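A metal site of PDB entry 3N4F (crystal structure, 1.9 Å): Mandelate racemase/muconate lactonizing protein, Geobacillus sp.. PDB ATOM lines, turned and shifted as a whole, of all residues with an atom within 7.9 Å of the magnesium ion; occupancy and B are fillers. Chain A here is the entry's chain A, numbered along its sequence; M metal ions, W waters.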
ATOM      1  N   ASN A 209      -6.407  12.610  19.151  1.00  0.00           N
ATOM      2  CA  ASN A 209      -7.398  13.171  18.241  1.00  0.00           C
ATOM      3  C   ASN A 209      -7.023  14.546  17.698  1.00  0.00           C
ATOM      4  O   ASN A 209      -7.859  15.451  17.691  1.00  0.00           O
ATOM      5  CB  ASN A 209      -8.791  13.168  18.892  1.00  0.00           C
ATOM      6  CG  ASN A 209      -9.387  11.767  18.924  1.00  0.00           C
ATOM      7  OD1 ASN A 209      -9.385  11.103  19.951  1.00  0.00           O
ATOM      8  ND2 ASN A 209      -9.808  11.280  17.755  1.00  0.00           N
ATOM      9  N   ASN A 210      -5.754  14.684  17.288  1.00  0.00           N
ATOM     10  CA  ASN A 210      -5.192  15.894  16.632  1.00  0.00           C
ATOM     11  C   ASN A 210      -5.015  17.159  17.506  1.00  0.00           C
ATOM     12  O   ASN A 210      -4.717  18.263  16.984  1.00  0.00           O
ATOM     13  CB  ASN A 210      -5.981  16.229  15.351  1.00  0.00           C
ATOM     14  CG  ASN A 210      -5.761  15.197  14.247  1.00  0.00           C
ATOM     15  OD1 ASN A 210      -4.792  14.451  14.269  1.00  0.00           O
ATOM     16  ND2 ASN A 210      -6.670  15.152  13.291  1.00  0.00           N
ATOM     17  N   GLU A 233      -0.977   8.010  18.209  1.00  0.00           N
ATOM     18  CA  GLU A 233      -1.979   8.043  17.152  1.00  0.00           C
ATOM     19  C   GLU A 233      -2.530   9.452  17.070  1.00  0.00           C
ATOM     20  O   GLU A 233      -2.976  10.011  18.083  1.00  0.00           O
ATOM     21  CB  GLU A 233      -3.084   7.060  17.502  1.00  0.00           C
ATOM     22  CG  GLU A 233      -4.403   7.259  16.747  1.00  0.00           C
ATOM     23  CD  GLU A 233      -5.378   6.119  16.992  1.00  0.00           C
ATOM     24  OE1 GLU A 233      -4.946   5.052  17.492  1.00  0.00           O
ATOM     25  OE2 GLU A 233      -6.567   6.291  16.651  1.00  0.00           O
ATOM     26  N   GLU A 234      -2.500  10.006  15.862  1.00  0.00           N
ATOM     27  CA  GLU A 234      -3.051  11.344  15.572  1.00  0.00           C
ATOM     28  C   GLU A 234      -2.670  12.384  16.620  1.00  0.00           C
ATOM     29  O   GLU A 234      -3.542  13.038  17.210  1.00  0.00           O
ATOM     30  CB  GLU A 234      -4.583  11.288  15.415  1.00  0.00           C
ATOM     31  CG  GLU A 234      -5.068  10.430  14.230  1.00  0.00           C
ATOM     32  CD  GLU A 234      -6.427  10.861  13.694  1.00  0.00           C
ATOM     33  OE1 GLU A 234      -7.398  10.937  14.486  1.00  0.00           O
ATOM     34  OE2 GLU A 234      -6.535  11.107  12.460  1.00  0.00           O
ATOM     35  N   ALA A 235      -1.370  12.561  16.823  1.00  0.00           N
ATOM     36  CA  ALA A 235      -0.837  13.670  17.623  1.00  0.00           C
ATOM     37  C   ALA A 235      -1.334  15.014  17.067  1.00  0.00           C
ATOM     38  O   ALA A 235      -1.688  15.936  17.826  1.00  0.00           O
ATOM     39  CB  ALA A 235       0.689  13.625  17.621  1.00  0.00           C
ATOM     40  N   PHE A 236      -1.347  15.121  15.743  1.00  0.00           N
ATOM     41  CA  PHE A 236      -1.789  16.336  15.036  1.00  0.00           C
ATOM     42  C   PHE A 236      -2.124  15.867  13.626  1.00  0.00           C
ATOM     43  O   PHE A 236      -1.663  14.799  13.222  1.00  0.00           O
ATOM     44  CB  PHE A 236      -0.694  17.392  15.009  1.00  0.00           C
ATOM     45  CG  PHE A 236       0.689  16.825  14.855  1.00  0.00           C
ATOM     46  CD1 PHE A 236       1.547  16.742  15.954  1.00  0.00           C
ATOM     47  CD2 PHE A 236       1.126  16.338  13.620  1.00  0.00           C
ATOM     48  CE1 PHE A 236       2.839  16.186  15.817  1.00  0.00           C
ATOM     49  CE2 PHE A 236       2.407  15.777  13.466  1.00  0.00           C
ATOM     50  CZ  PHE A 236       3.265  15.694  14.565  1.00  0.00           C
ATOM     51  N   HIS A 237      -2.891  16.637  12.867  1.00  0.00           N
ATOM     52  CA  HIS A 237      -3.282  16.145  11.535  1.00  0.00           C
ATOM     53  C   HIS A 237      -2.012  15.789  10.755  1.00  0.00           C
ATOM     54  O   HIS A 237      -1.026  16.523  10.809  1.00  0.00           O
ATOM     55  CB  HIS A 237      -4.091  17.188  10.753  1.00  0.00           C
ATOM     56  CG  HIS A 237      -4.520  16.686   9.412  1.00  0.00           C
ATOM     57  ND1 HIS A 237      -5.388  15.621   9.278  1.00  0.00           N
ATOM     58  CD2 HIS A 237      -4.159  17.055   8.167  1.00  0.00           C
ATOM     59  CE1 HIS A 237      -5.546  15.367   7.985  1.00  0.00           C
ATOM     60  NE2 HIS A 237      -4.828  16.226   7.292  1.00  0.00           N
ATOM     61  N   GLU A 238      -2.028  14.643  10.061  1.00  0.00           N
ATOM     62  CA  GLU A 238      -0.798  14.107   9.457  1.00  0.00           C
ATOM     63  C   GLU A 238      -0.131  15.133   8.550  1.00  0.00           C
ATOM     64  O   GLU A 238      -0.810  15.834   7.782  1.00  0.00           O
ATOM     65  CB  GLU A 238      -1.060  12.809   8.682  1.00  0.00           C
ATOM     66  CG  GLU A 238      -2.271  12.879   7.743  1.00  0.00           C
ATOM     67  CD  GLU A 238      -3.579  12.357   8.380  1.00  0.00           C
ATOM     68  OE1 GLU A 238      -4.392  11.813   7.614  1.00  0.00           O
ATOM     69  OE2 GLU A 238      -3.802  12.497   9.614  1.00  0.00           O
ATOM     70  N   ASP A 239       1.194  15.214   8.669  1.00  0.00           N
ATOM     71  CA  ASP A 239       2.006  16.186   7.945  1.00  0.00           C
ATOM     72  C   ASP A 239       3.374  15.535   7.790  1.00  0.00           C
ATOM     73  O   ASP A 239       4.002  15.212   8.789  1.00  0.00           O
ATOM     74  CB  ASP A 239       2.107  17.508   8.739  1.00  0.00           C
ATOM     75  CG  ASP A 239       2.915  18.590   8.020  1.00  0.00           C
ATOM     76  OD1 ASP A 239       3.985  18.266   7.461  1.00  0.00           O
ATOM     77  OD2 ASP A 239       2.483  19.766   8.009  1.00  0.00           O
ATOM     78  N   TYR A 243       6.115  14.792  10.883  1.00  0.00           N
ATOM     79  CA  TYR A 243       6.305  13.388  11.245  1.00  0.00           C
ATOM     80  C   TYR A 243       7.742  12.889  10.977  1.00  0.00           C
ATOM     81  O   TYR A 243       8.220  11.995  11.661  1.00  0.00           O
ATOM     82  CB  TYR A 243       5.326  12.499  10.494  1.00  0.00           C
ATOM     83  CG  TYR A 243       3.991  12.297  11.195  1.00  0.00           C
ATOM     84  CD1 TYR A 243       3.876  12.369  12.578  1.00  0.00           C
ATOM     85  CD2 TYR A 243       2.857  11.975  10.450  1.00  0.00           C
ATOM     86  CE1 TYR A 243       2.649  12.146  13.218  1.00  0.00           C
ATOM     87  CE2 TYR A 243       1.628  11.741  11.071  1.00  0.00           C
ATOM     88  CZ  TYR A 243       1.531  11.833  12.461  1.00  0.00           C
ATOM     89  OH  TYR A 243       0.322  11.590  13.084  1.00  0.00           O
ATOM     90  N   ALA A 260       0.933   6.197  14.364  1.00  0.00           N
ATOM     91  CA  ALA A 260      -0.299   5.644  13.787  1.00  0.00           C
ATOM     92  C   ALA A 260      -1.173   6.771  13.298  1.00  0.00           C
ATOM     93  O   ALA A 260      -1.304   7.791  13.976  1.00  0.00           O
ATOM     94  CB  ALA A 260      -1.067   4.794  14.835  1.00  0.00           C
ATOM     95  N   ASP A 261      -1.780   6.585  12.127  1.00  0.00           N
ATOM     96  CA  ASP A 261      -2.695   7.613  11.634  1.00  0.00           C
ATOM     97  C   ASP A 261      -3.582   7.002  10.559  1.00  0.00           C
ATOM     98  O   ASP A 261      -3.386   5.846  10.175  1.00  0.00           O
ATOM     99  CB  ASP A 261      -1.885   8.788  11.079  1.00  0.00           C
ATOM    100  CG  ASP A 261      -2.541  10.140  11.345  1.00  0.00           C
ATOM    101  OD1 ASP A 261      -3.765  10.263  11.162  1.00  0.00           O
ATOM    102  OD2 ASP A 261      -1.823  11.075  11.758  1.00  0.00           O
ATOM    103  N   GLY A 262      -4.570   7.760  10.096  1.00  0.00           N
ATOM    104  CA  GLY A 262      -5.365   7.338   8.967  1.00  0.00           C
ATOM    105  C   GLY A 262      -6.871   7.334   9.093  1.00  0.00           C
ATOM    106  O   GLY A 262      -7.569   7.206   8.093  1.00  0.00           O
ATOM    107  N   GLU A 263      -7.398   7.482  10.318  1.00  0.00           N
ATOM    108  CA  GLU A 263      -8.858   7.528  10.461  1.00  0.00           C
ATOM    109  C   GLU A 263      -9.442   8.840   9.920  1.00  0.00           C
ATOM    110  O   GLU A 263      -8.703   9.786   9.600  1.00  0.00           O
ATOM    111  CB  GLU A 263      -9.289   7.248  11.903  1.00  0.00           C
ATOM    112  CG  GLU A 263      -9.097   8.427  12.819  1.00  0.00           C
ATOM    113  CD  GLU A 263      -9.476   8.105  14.242  1.00  0.00           C
ATOM    114  OE1 GLU A 263     -10.480   8.686  14.706  1.00  0.00           O
ATOM    115  OE2 GLU A 263      -8.776   7.286  14.889  1.00  0.00           O
ATOM    116  N   GLY A 264     -10.767   8.886   9.774  1.00  0.00           N
ATOM    117  CA  GLY A 264     -11.457  10.127   9.356  1.00  0.00           C
ATOM    118  C   GLY A 264     -11.061  10.661   7.990  1.00  0.00           C
ATOM    119  O   GLY A 264     -10.863   9.893   7.049  1.00  0.00           O
ATOM    120  N   LEU A 265     -10.977  11.978   7.873  1.00  0.00           N
ATOM    121  CA  LEU A 265     -10.631  12.635   6.610  1.00  0.00           C
ATOM    122  C   LEU A 265      -9.117  12.690   6.427  1.00  0.00           C
ATOM    123  O   LEU A 265      -8.498  13.746   6.596  1.00  0.00           O
ATOM    124  CB  LEU A 265     -11.209  14.053   6.579  1.00  0.00           C
ATOM    125  CG  LEU A 265     -12.534  14.344   5.860  1.00  0.00           C
ATOM    126  CD1 LEU A 265     -13.497  13.143   5.838  1.00  0.00           C
ATOM    127  CD2 LEU A 265     -13.186  15.588   6.449  1.00  0.00           C
ATOM    128  N   ALA A 266      -8.534  11.557   6.028  1.00  0.00           N
ATOM    129  CA  ALA A 266      -7.082  11.414   5.932  1.00  0.00           C
ATOM    130  C   ALA A 266      -6.486  12.158   4.756  1.00  0.00           C
ATOM    131  O   ALA A 266      -7.148  12.356   3.719  1.00  0.00           O
ATOM    132  CB  ALA A 266      -6.700   9.943   5.834  1.00  0.00           C
ATOM    133  N   SER A 267      -5.222  12.562   4.910  1.00  0.00           N
ATOM    134  CA  SER A 267      -4.438  13.101   3.826  1.00  0.00           C
ATOM    135  C   SER A 267      -4.452  12.112   2.646  1.00  0.00           C
ATOM    136  O   SER A 267      -4.286  10.903   2.842  1.00  0.00           O
ATOM    137  CB  SER A 267      -3.004  13.324   4.295  1.00  0.00           C
ATOM    138  OG  SER A 267      -2.129  13.445   3.175  1.00  0.00           O
ATOM    139  N   LEU A 270      -1.168  10.082   2.585  1.00  0.00           N
ATOM    140  CA  LEU A 270      -0.725   9.389   3.787  1.00  0.00           C
ATOM    141  C   LEU A 270       0.056   8.090   3.488  1.00  0.00           C
ATOM    142  O   LEU A 270       1.038   7.823   4.131  1.00  0.00           O
ATOM    143  CB  LEU A 270      -1.898   9.101   4.718  1.00  0.00           C
ATOM    144  CG  LEU A 270      -1.535   8.431   6.048  1.00  0.00           C
ATOM    145  CD1 LEU A 270      -0.566   9.283   6.853  1.00  0.00           C
ATOM    146  CD2 LEU A 270      -2.781   8.065   6.877  1.00  0.00           C
ATOM    147  N   GLN A 283      -4.646   3.273   9.700  1.00  0.00           N
ATOM    148  CA  GLN A 283      -5.869   3.063  10.504  1.00  0.00           C
ATOM    149  C   GLN A 283      -7.203   3.389   9.829  1.00  0.00           C
ATOM    150  O   GLN A 283      -8.176   3.783  10.500  1.00  0.00           O
ATOM    151  CB  GLN A 283      -5.781   3.827  11.829  1.00  0.00           C
ATOM    152  CG  GLN A 283      -4.622   3.416  12.687  1.00  0.00           C
ATOM    153  CD  GLN A 283      -4.546   4.212  13.949  1.00  0.00           C
ATOM    154  OE1 GLN A 283      -4.363   5.428  13.924  1.00  0.00           O
ATOM    155  NE2 GLN A 283      -4.667   3.529  15.082  1.00  0.00           N
HETATM  156 MG    MG M   1      -5.068  11.741  11.061  1.00  0.00          MG
HETATM  157  O   HOH W   1      -6.090  10.720   9.466  1.00  0.00           O
HETATM  158  O   HOH W   2      -4.010  12.834  12.453  1.00  0.00           O
HETATM  159  O   HOH W   3      -6.187  13.547  10.854  1.00  0.00           O
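The backbone carbonyl oxygen (O) of Glu 234 sits at hydrogen-bond distance from the backbone NH (N) of Asn 210, at 2.8 Å. N of Gln 283 is in hydrogen-bond range of O of Asp 261, at 2.9 Å. The side-chain carboxylate (OE1) of Glu 238 sits at hydrogen-bond distance from the backbone NH (N) of Ser 267. O of Glu 234 is in hydrogen-bond range of N of Asn 209, 3.5 Å away. The side-chain carboxylate of Asp 261 sits at hydrogen-bond distance from the side-chain hydroxyl of Tyr 243, 2.6 Å away. The backbone NH (N) of Glu 234 lies within hydrogen-bond range of the backbone carbonyl oxygen (O) of Ala 260, at 3.1 Å.
Within 4 Å of the magnesium ion: Glu 234, Glu 238 and Asp 261. The nearest printed residue that does not touch the magnesium ion is Gly 262 (4.1 Å).
The side-chain carboxylate (OD1) of Asp 261 binds the magnesium ion. The magnesium ion is bound by water W2 (2.1 Å). OE2 of Glu 238 binds the magnesium ion (2.1 Å). The magnesium ion is bound by OE2 of Glu 234 (2.1 Å). The magnesium ion is bound by water W3 (2.1 Å). Water W1 binds the magnesium ion, 2.2 Å away. The magnesium ion has six donor atoms within binding distance.
Water W1 lies within hydrogen-bond range of the side-chain carboxylate (OE1) of Glu 238 (2.7 Å), the backbone carbonyl oxygen (O) of Glu 263 (2.8 Å) and the backbone NH (N) of Gly 262 (3.4 Å). Water W3 bridges a ring nitrogen (ND1) of His 237 and the side-chain amide nitrogen of Asn 210.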
